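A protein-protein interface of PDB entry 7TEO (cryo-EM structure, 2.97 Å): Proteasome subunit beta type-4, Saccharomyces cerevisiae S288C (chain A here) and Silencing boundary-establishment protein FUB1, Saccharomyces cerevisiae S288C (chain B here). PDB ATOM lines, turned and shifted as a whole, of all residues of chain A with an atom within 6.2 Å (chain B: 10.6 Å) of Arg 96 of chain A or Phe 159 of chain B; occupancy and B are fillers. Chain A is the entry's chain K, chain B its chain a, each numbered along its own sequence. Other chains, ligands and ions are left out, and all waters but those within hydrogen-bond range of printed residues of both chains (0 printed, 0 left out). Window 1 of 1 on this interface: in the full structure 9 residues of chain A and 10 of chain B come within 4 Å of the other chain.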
ATOM      1  N   ASP A  52       6.129 -35.479  16.202  1.00  0.00           N
ATOM      2  CA  ASP A  52       7.167 -35.834  17.161  1.00  0.00           C
ATOM      3  C   ASP A  52       6.786 -37.080  17.942  1.00  0.00           C
ATOM      4  O   ASP A  52       7.619 -37.967  18.151  1.00  0.00           O
ATOM      5  CB  ASP A  52       7.420 -34.670  18.119  1.00  0.00           C
ATOM      6  CG  ASP A  52       8.021 -33.466  17.428  1.00  0.00           C
ATOM      7  OD1 ASP A  52       8.495 -33.611  16.284  1.00  0.00           O
ATOM      8  OD2 ASP A  52       8.017 -32.373  18.032  1.00  0.00           O
ATOM      9  N   SER A  91      17.831 -34.421  23.295  1.00  0.00           N
ATOM     10  CA  SER A  91      17.131 -33.749  22.207  1.00  0.00           C
ATOM     11  C   SER A  91      16.905 -32.263  22.467  1.00  0.00           C
ATOM     12  O   SER A  91      17.004 -31.462  21.533  1.00  0.00           O
ATOM     13  CB  SER A  91      15.786 -34.430  21.954  1.00  0.00           C
ATOM     14  OG  SER A  91      14.805 -33.964  22.861  1.00  0.00           O
ATOM     15  N   ILE A  92      16.604 -31.871  23.708  1.00  0.00           N
ATOM     16  CA  ILE A  92      16.137 -30.508  23.961  1.00  0.00           C
ATOM     17  C   ILE A  92      17.170 -29.445  23.628  1.00  0.00           C
ATOM     18  O   ILE A  92      16.791 -28.304  23.346  1.00  0.00           O
ATOM     19  CB  ILE A  92      15.697 -30.319  25.427  1.00  0.00           C
ATOM     20  CG1 ILE A  92      16.852 -30.610  26.386  1.00  0.00           C
ATOM     21  CG2 ILE A  92      14.512 -31.211  25.736  1.00  0.00           C
ATOM     22  CD1 ILE A  92      16.537 -30.277  27.824  1.00  0.00           C
ATOM     23  N   SER A  94      19.370 -29.974  21.106  1.00  0.00           N
ATOM     24  CA  SER A  94      19.651 -30.136  19.693  1.00  0.00           C
ATOM     25  C   SER A  94      18.761 -29.208  18.870  1.00  0.00           C
ATOM     26  O   SER A  94      17.956 -28.441  19.401  1.00  0.00           O
ATOM     27  CB  SER A  94      19.445 -31.588  19.267  1.00  0.00           C
ATOM     28  OG  SER A  94      18.078 -31.852  19.007  1.00  0.00           O
ATOM     29  N   ARG A  95      18.919 -29.287  17.549  1.00  0.00           N
ATOM     30  CA  ARG A  95      18.153 -28.418  16.663  1.00  0.00           C
ATOM     31  C   ARG A  95      16.663 -28.728  16.711  1.00  0.00           C
ATOM     32  O   ARG A  95      15.838 -27.812  16.621  1.00  0.00           O
ATOM     33  CB  ARG A  95      18.676 -28.543  15.232  1.00  0.00           C
ATOM     34  CG  ARG A  95      18.169 -27.466  14.284  1.00  0.00           C
ATOM     35  CD  ARG A  95      18.284 -27.911  12.836  1.00  0.00           C
ATOM     36  NE  ARG A  95      17.158 -28.748  12.433  1.00  0.00           N
ATOM     37  CZ  ARG A  95      17.250 -29.831  11.671  1.00  0.00           C
ATOM     38  NH1 ARG A  95      18.411 -30.245  11.187  1.00  0.00           N
ATOM     39  NH2 ARG A  95      16.148 -30.518  11.387  1.00  0.00           N
ATOM     40  N   ARG A  96      16.297 -30.004  16.849  1.00  0.00           N
ATOM     41  CA  ARG A  96      14.905 -30.448  16.777  1.00  0.00           C
ATOM     42  C   ARG A  96      14.550 -31.236  18.031  1.00  0.00           C
ATOM     43  O   ARG A  96      14.683 -32.470  18.060  1.00  0.00           O
ATOM     44  CB  ARG A  96      14.671 -31.283  15.518  1.00  0.00           C
ATOM     45  CG  ARG A  96      13.253 -31.816  15.363  1.00  0.00           C
ATOM     46  CD  ARG A  96      12.263 -30.681  15.169  1.00  0.00           C
ATOM     47  NE  ARG A  96      12.488 -29.963  13.921  1.00  0.00           N
ATOM     48  CZ  ARG A  96      11.929 -28.799  13.617  1.00  0.00           C
ATOM     49  NH1 ARG A  96      11.095 -28.195  14.447  1.00  0.00           N
ATOM     50  NH2 ARG A  96      12.222 -28.224  12.455  1.00  0.00           N
ATOM     51  N   PRO A  97      14.106 -30.567  19.093  1.00  0.00           N
ATOM     52  CA  PRO A  97      13.638 -31.292  20.278  1.00  0.00           C
ATOM     53  C   PRO A  97      12.374 -32.089  19.996  1.00  0.00           C
ATOM     54  O   PRO A  97      11.564 -31.733  19.137  1.00  0.00           O
ATOM     55  CB  PRO A  97      13.369 -30.174  21.293  1.00  0.00           C
ATOM     56  CG  PRO A  97      14.192 -29.034  20.823  1.00  0.00           C
ATOM     57  CD  PRO A  97      14.158 -29.116  19.334  1.00  0.00           C
ATOM     58  N   TYR A  98      12.210 -33.181  20.739  1.00  0.00           N
ATOM     59  CA  TYR A  98      10.966 -33.942  20.740  1.00  0.00           C
ATOM     60  C   TYR A  98      10.067 -33.382  21.834  1.00  0.00           C
ATOM     61  O   TYR A  98      10.374 -33.509  23.024  1.00  0.00           O
ATOM     62  CB  TYR A  98      11.223 -35.428  20.973  1.00  0.00           C
ATOM     63  CG  TYR A  98      12.198 -36.067  20.017  1.00  0.00           C
ATOM     64  CD1 TYR A  98      11.812 -36.420  18.733  1.00  0.00           C
ATOM     65  CD2 TYR A  98      13.503 -36.341  20.406  1.00  0.00           C
ATOM     66  CE1 TYR A  98      12.699 -37.015  17.859  1.00  0.00           C
ATOM     67  CE2 TYR A  98      14.396 -36.936  19.541  1.00  0.00           C
ATOM     68  CZ  TYR A  98      13.989 -37.270  18.268  1.00  0.00           C
ATOM     69  OH  TYR A  98      14.876 -37.863  17.402  1.00  0.00           O
ATOM     70  N   GLN A  99       8.959 -32.761  21.436  1.00  0.00           N
ATOM     71  CA  GLN A  99       7.954 -32.288  22.387  1.00  0.00           C
ATOM     72  C   GLN A  99       7.017 -33.450  22.716  1.00  0.00           C
ATOM     73  O   GLN A  99       5.832 -33.462  22.377  1.00  0.00           O
ATOM     74  CB  GLN A  99       7.202 -31.098  21.812  1.00  0.00           C
ATOM     75  CG  GLN A  99       8.053 -29.860  21.593  1.00  0.00           C
ATOM     76  CD  GLN A  99       8.629 -29.308  22.880  1.00  0.00           C
ATOM     77  OE1 GLN A  99       9.831 -29.398  23.123  1.00  0.00           O
ATOM     78  NE2 GLN A  99       7.772 -28.727  23.710  1.00  0.00           N
ATOM     79  N   ALA B 144      15.989 -11.524  15.087  1.00  0.00           N
ATOM     80  CA  ALA B 144      15.080 -12.266  15.958  1.00  0.00           C
ATOM     81  C   ALA B 144      15.342 -11.930  17.415  1.00  0.00           C
ATOM     82  O   ALA B 144      16.470 -11.587  17.785  1.00  0.00           O
ATOM     83  CB  ALA B 144      15.217 -13.757  15.706  1.00  0.00           C
ATOM     84  N   PRO B 145      14.316 -12.032  18.250  1.00  0.00           N
ATOM     85  CA  PRO B 145      14.515 -11.754  19.673  1.00  0.00           C
ATOM     86  C   PRO B 145      15.394 -12.815  20.321  1.00  0.00           C
ATOM     87  O   PRO B 145      15.420 -13.979  19.911  1.00  0.00           O
ATOM     88  CB  PRO B 145      13.087 -11.780  20.258  1.00  0.00           C
ATOM     89  CG  PRO B 145      12.342 -12.670  19.352  1.00  0.00           C
ATOM     90  CD  PRO B 145      12.927 -12.461  17.974  1.00  0.00           C
ATOM     91  N   LEU B 146      16.150 -12.388  21.326  1.00  0.00           N
ATOM     92  CA  LEU B 146      17.099 -13.268  22.005  1.00  0.00           C
ATOM     93  C   LEU B 146      16.362 -14.318  22.835  1.00  0.00           C
ATOM     94  O   LEU B 146      15.370 -14.025  23.513  1.00  0.00           O
ATOM     95  CB  LEU B 146      18.034 -12.467  22.907  1.00  0.00           C
ATOM     96  CG  LEU B 146      19.143 -11.681  22.200  1.00  0.00           C
ATOM     97  CD1 LEU B 146      20.078 -11.069  23.224  1.00  0.00           C
ATOM     98  CD2 LEU B 146      19.925 -12.549  21.231  1.00  0.00           C
ATOM     99  N   ASN B 147      16.871 -15.540  22.804  1.00  0.00           N
ATOM    100  CA  ASN B 147      16.342 -16.607  23.634  1.00  0.00           C
ATOM    101  C   ASN B 147      16.606 -16.259  25.093  1.00  0.00           C
ATOM    102  O   ASN B 147      17.772 -16.080  25.473  1.00  0.00           O
ATOM    103  CB  ASN B 147      16.997 -17.936  23.264  1.00  0.00           C
ATOM    104  CG  ASN B 147      16.473 -19.102  24.079  1.00  0.00           C
ATOM    105  OD1 ASN B 147      15.679 -18.924  25.000  1.00  0.00           O
ATOM    106  ND2 ASN B 147      16.923 -20.304  23.743  1.00  0.00           N
ATOM    107  N   PRO B 148      15.577 -16.152  25.939  1.00  0.00           N
ATOM    108  CA  PRO B 148      15.838 -15.764  27.334  1.00  0.00           C
ATOM    109  C   PRO B 148      16.734 -16.742  28.068  1.00  0.00           C
ATOM    110  O   PRO B 148      17.413 -16.346  29.022  1.00  0.00           O
ATOM    111  CB  PRO B 148      14.433 -15.703  27.947  1.00  0.00           C
ATOM    112  CG  PRO B 148      13.604 -16.589  27.091  1.00  0.00           C
ATOM    113  CD  PRO B 148      14.148 -16.422  25.707  1.00  0.00           C
ATOM    114  N   GLY B 151      20.890 -21.888  24.972  1.00  0.00           N
ATOM    115  CA  GLY B 151      21.132 -23.326  24.936  1.00  0.00           C
ATOM    116  C   GLY B 151      19.877 -24.155  24.762  1.00  0.00           C
ATOM    117  O   GLY B 151      19.841 -25.059  23.928  1.00  0.00           O
ATOM    118  N   LEU B 152      18.838 -23.854  25.536  1.00  0.00           N
ATOM    119  CA  LEU B 152      17.575 -24.578  25.434  1.00  0.00           C
ATOM    120  C   LEU B 152      16.844 -24.142  24.173  1.00  0.00           C
ATOM    121  O   LEU B 152      16.380 -23.002  24.076  1.00  0.00           O
ATOM    122  CB  LEU B 152      16.716 -24.324  26.669  1.00  0.00           C
ATOM    123  CG  LEU B 152      17.191 -24.970  27.970  1.00  0.00           C
ATOM    124  CD1 LEU B 152      16.258 -24.599  29.106  1.00  0.00           C
ATOM    125  CD2 LEU B 152      17.280 -26.479  27.825  1.00  0.00           C
ATOM    126  N   THR B 153      16.737 -25.050  23.202  1.00  0.00           N
ATOM    127  CA  THR B 153      16.024 -24.744  21.970  1.00  0.00           C
ATOM    128  C   THR B 153      14.514 -24.809  22.137  1.00  0.00           C
ATOM    129  O   THR B 153      13.788 -24.296  21.278  1.00  0.00           O
ATOM    130  CB  THR B 153      16.464 -25.696  20.856  1.00  0.00           C
ATOM    131  OG1 THR B 153      16.233 -27.049  21.259  1.00  0.00           O
ATOM    132  CG2 THR B 153      17.943 -25.505  20.544  1.00  0.00           C
ATOM    133  N   VAL B 154      14.021 -25.422  23.214  1.00  0.00           N
ATOM    134  CA  VAL B 154      12.592 -25.438  23.489  1.00  0.00           C
ATOM    135  C   VAL B 154      12.049 -24.052  23.799  1.00  0.00           C
ATOM    136  O   VAL B 154      10.830 -23.859  23.803  1.00  0.00           O
ATOM    137  CB  VAL B 154      12.278 -26.407  24.651  1.00  0.00           C
ATOM    138  CG1 VAL B 154      12.550 -27.842  24.232  1.00  0.00           C
ATOM    139  CG2 VAL B 154      13.087 -26.049  25.891  1.00  0.00           C
ATOM    140  N   THR B 155      12.926 -23.080  24.061  1.00  0.00           N
ATOM    141  CA  THR B 155      12.522 -21.701  24.315  1.00  0.00           C
ATOM    142  C   THR B 155      12.986 -20.751  23.219  1.00  0.00           C
ATOM    143  O   THR B 155      12.813 -19.535  23.354  1.00  0.00           O
ATOM    144  CB  THR B 155      13.059 -21.228  25.669  1.00  0.00           C
ATOM    145  OG1 THR B 155      14.482 -21.388  25.706  1.00  0.00           O
ATOM    146  CG2 THR B 155      12.433 -22.020  26.805  1.00  0.00           C
ATOM    147  N   GLU B 156      13.573 -21.265  22.145  1.00  0.00           N
ATOM    148  CA  GLU B 156      13.981 -20.407  21.041  1.00  0.00           C
ATOM    149  C   GLU B 156      12.749 -19.792  20.386  1.00  0.00           C
ATOM    150  O   GLU B 156      11.774 -20.505  20.123  1.00  0.00           O
ATOM    151  CB  GLU B 156      14.785 -21.196  20.013  1.00  0.00           C
ATOM    152  CG  GLU B 156      16.216 -21.474  20.436  1.00  0.00           C
ATOM    153  CD  GLU B 156      17.128 -20.281  20.237  1.00  0.00           C
ATOM    154  OE1 GLU B 156      16.849 -19.459  19.339  1.00  0.00           O
ATOM    155  OE2 GLU B 156      18.125 -20.167  20.980  1.00  0.00           O
ATOM    156  N   PRO B 157      12.744 -18.483  20.115  1.00  0.00           N
ATOM    157  CA  PRO B 157      11.570 -17.895  19.448  1.00  0.00           C
ATOM    158  C   PRO B 157      11.243 -18.551  18.116  1.00  0.00           C
ATOM    159  O   PRO B 157      10.063 -18.725  17.791  1.00  0.00           O
ATOM    160  CB  PRO B 157      11.971 -16.423  19.282  1.00  0.00           C
ATOM    161  CG  PRO B 157      12.960 -16.184  20.366  1.00  0.00           C
ATOM    162  CD  PRO B 157      13.734 -17.456  20.484  1.00  0.00           C
ATOM    163  N   SER B 158      12.258 -18.922  17.332  1.00  0.00           N
ATOM    164  CA  SER B 158      12.009 -19.552  16.040  1.00  0.00           C
ATOM    165  C   SER B 158      11.407 -20.942  16.180  1.00  0.00           C
ATOM    166  O   SER B 158      10.787 -21.434  15.231  1.00  0.00           O
ATOM    167  CB  SER B 158      13.306 -19.636  15.238  1.00  0.00           C
ATOM    168  OG  SER B 158      14.230 -20.509  15.862  1.00  0.00           O
ATOM    169  N   PHE B 159      11.575 -21.583  17.333  1.00  0.00           N
ATOM    170  CA  PHE B 159      11.004 -22.898  17.598  1.00  0.00           C
ATOM    171  C   PHE B 159       9.689 -22.820  18.360  1.00  0.00           C
ATOM    172  O   PHE B 159       8.783 -23.619  18.108  1.00  0.00           O
ATOM    173  CB  PHE B 159      12.000 -23.754  18.383  1.00  0.00           C
ATOM    174  CG  PHE B 159      11.498 -25.131  18.699  1.00  0.00           C
ATOM    175  CD1 PHE B 159      11.536 -26.133  17.744  1.00  0.00           C
ATOM    176  CD2 PHE B 159      10.987 -25.423  19.949  1.00  0.00           C
ATOM    177  CE1 PHE B 159      11.073 -27.397  18.035  1.00  0.00           C
ATOM    178  CE2 PHE B 159      10.524 -26.685  20.245  1.00  0.00           C
ATOM    179  CZ  PHE B 159      10.567 -27.674  19.288  1.00  0.00           C
ATOM    180  N   ALA B 160       9.570 -21.876  19.297  1.00  0.00           N
ATOM    181  CA  ALA B 160       8.302 -21.661  19.985  1.00  0.00           C
ATOM    182  C   ALA B 160       7.250 -21.066  19.060  1.00  0.00           C
ATOM    183  O   ALA B 160       6.056 -21.339  19.229  1.00  0.00           O
ATOM    184  CB  ALA B 160       8.510 -20.746  21.193  1.00  0.00           C
ATOM    185  N   ASN B 161       7.662 -20.239  18.100  1.00  0.00           N
ATOM    186  CA  ASN B 161       6.748 -19.619  17.139  1.00  0.00           C
ATOM    187  C   ASN B 161       7.304 -19.786  15.732  1.00  0.00           C
ATOM    188  O   ASN B 161       7.814 -18.830  15.129  1.00  0.00           O
ATOM    189  CB  ASN B 161       6.542 -18.142  17.488  1.00  0.00           C
ATOM    190  CG  ASN B 161       5.968 -17.947  18.872  1.00  0.00           C
ATOM    191  OD1 ASN B 161       6.699 -17.668  19.826  1.00  0.00           O
ATOM    192  ND2 ASN B 161       4.656 -18.092  18.994  1.00  0.00           N
ATOM    193  N   PRO B 162       7.221 -20.998  15.166  1.00  0.00           N
ATOM    194  CA  PRO B 162       7.771 -21.216  13.820  1.00  0.00           C
ATOM    195  C   PRO B 162       7.069 -20.431  12.723  1.00  0.00           C
ATOM    196  O   PRO B 162       7.681 -20.240  11.665  1.00  0.00           O
ATOM    197  CB  PRO B 162       7.587 -22.721  13.604  1.00  0.00           C
ATOM    198  CG  PRO B 162       7.534 -23.285  14.959  1.00  0.00           C
ATOM    199  CD  PRO B 162       6.828 -22.273  15.792  1.00  0.00           C
ATOM    200  N   ALA B 163       5.816 -20.004  12.920  1.00  0.00           N
ATOM    201  CA  ALA B 163       5.088 -19.177  11.943  1.00  0.00           C
ATOM    202  C   ALA B 163       4.655 -19.969  10.703  1.00  0.00           C
ATOM    203  O   ALA B 163       4.465 -19.407   9.621  1.00  0.00           O
ATOM    204  CB  ALA B 163       5.915 -17.952  11.530  1.00  0.00           C
ATOM    205  N   GLY B 164       4.494 -21.277  10.846  1.00  0.00           N
ATOM    206  CA  GLY B 164       3.807 -22.069   9.842  1.00  0.00           C
ATOM    207  C   GLY B 164       4.463 -22.032   8.474  1.00  0.00           C
ATOM    208  O   GLY B 164       5.686 -21.936   8.333  1.00  0.00           O
ATOM    209  N   HIS B 178      -3.842 -24.439  14.754  1.00  0.00           N
ATOM    210  CA  HIS B 178      -4.103 -24.417  16.192  1.00  0.00           C
ATOM    211  C   HIS B 178      -4.982 -23.219  16.517  1.00  0.00           C
ATOM    212  O   HIS B 178      -4.481 -22.130  16.829  1.00  0.00           O
ATOM    213  CB  HIS B 178      -2.798 -24.368  16.986  1.00  0.00           C
ATOM    214  CG  HIS B 178      -1.860 -25.491  16.671  1.00  0.00           C
ATOM    215  ND1 HIS B 178      -0.831 -25.368  15.763  1.00  0.00           N
ATOM    216  CD2 HIS B 178      -1.800 -26.761  17.139  1.00  0.00           C
ATOM    217  CE1 HIS B 178      -0.175 -26.513  15.686  1.00  0.00           C
ATOM    218  NE2 HIS B 178      -0.744 -27.374  16.511  1.00  0.00           N
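No residue of chain B comes within 4 Å of Ser 91 of chain A.
Printed residues of chain B within 4 Å of Ile 92 of chain A: Leu 152, Thr 153 and Val 154.
Ser 94 of chain A touches one residue of chain B.
Arg 96 of chain A touches just one residue of chain B: Phe 159 (3.7 Å).
Of the printed residues of chain B, Pro 97 of chain A touches Thr 153, Val 154 and Phe 159.
Printed residues of chain B within 4 Å of Gln 99 of chain A: Val 154 (3.3 Å).
Leu 146 of chain B touches none of the printed residues of chain A.
Of the printed residues of chain A, Val 154 of chain B touches Ile 92, Pro 97 and Gln 99.
Printed residues of chain A within 4 Å of Phe 159 of chain B: Arg 96 (3.7 Å) and Pro 97 (3.8 Å).
The nearest residue of chain B that does not touch Arg 96 of chain A is Thr 153 of chain B (5.3 Å).
The nearest printed residue of chain B that does not touch Gln 99 of chain A is Phe 159 of chain B (4.02 Å).
Printed residues of chain A that touch a printed residue of chain B: Ile 92, Ser 94, Arg 96, Pro 97 and Gln 99.
Hydrophobic or aromatic side chains of chain A that line the printed part of chain B: Ile 92 and Pro 97.
Along chain A the printed residues that touch a printed residue of chain B span positions 92 to 99.
Printed residues of chain B that touch a printed residue of chain A: Leu 152, Thr 153, Val 154 and Phe 159.
Among the printed residues, 9 pairs touch across the chains.
Among the printed residues, no Asp or Glu carboxylate lies within 4 Å of a Lys or Arg side-chain nitrogen of the other chain.
OG1 of Thr 153 of chain B is in hydrogen-bond range of O of Ile 92 of chain A.
The backbone carbonyl oxygen (O) of Ser 94 of chain A sits at hydrogen-bond distance from the side-chain hydroxyl (OG1) of Thr 153 of chain B (2.9 Å).
Among the printed residues, pairs that only touch across the chains: Ile 92 of chain A with Leu 152 of chain B (3.9 Å), Ile 92 of chain A with Val 154 of chain B (3.9995 Å), Arg 96 of chain A with Phe 159 of chain B (3.7 Å), Pro 97 of chain A with Thr 153 of chain B (2.9 Å), Pro 97 of chain A with Val 154 of chain B (3.8 Å), Pro 97 of chain A with Phe 159 of chain B (3.8 Å) and Gln 99 of chain A with Val 154 of chain B (3.3 Å).
The backbone carbonyl oxygen of Leu 152 of chain B lies within hydrogen-bond range of the side-chain hydroxyl of Thr 155 of chain B, at 3.0 Å.
N of Arg 96 of chain A lies close to OG of Ser 94 of chain A (3.4 Å).
The backbone carbonyl oxygen of Ser 91 of chain A lies within hydrogen-bond range of the side-chain hydroxyl of Ser 94 of chain A (2.8 Å).
The backbone carbonyl oxygen of Leu 152 of chain B is in hydrogen-bond range of the side-chain amide nitrogen of Asn 147 of chain B, at 2.8 Å.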
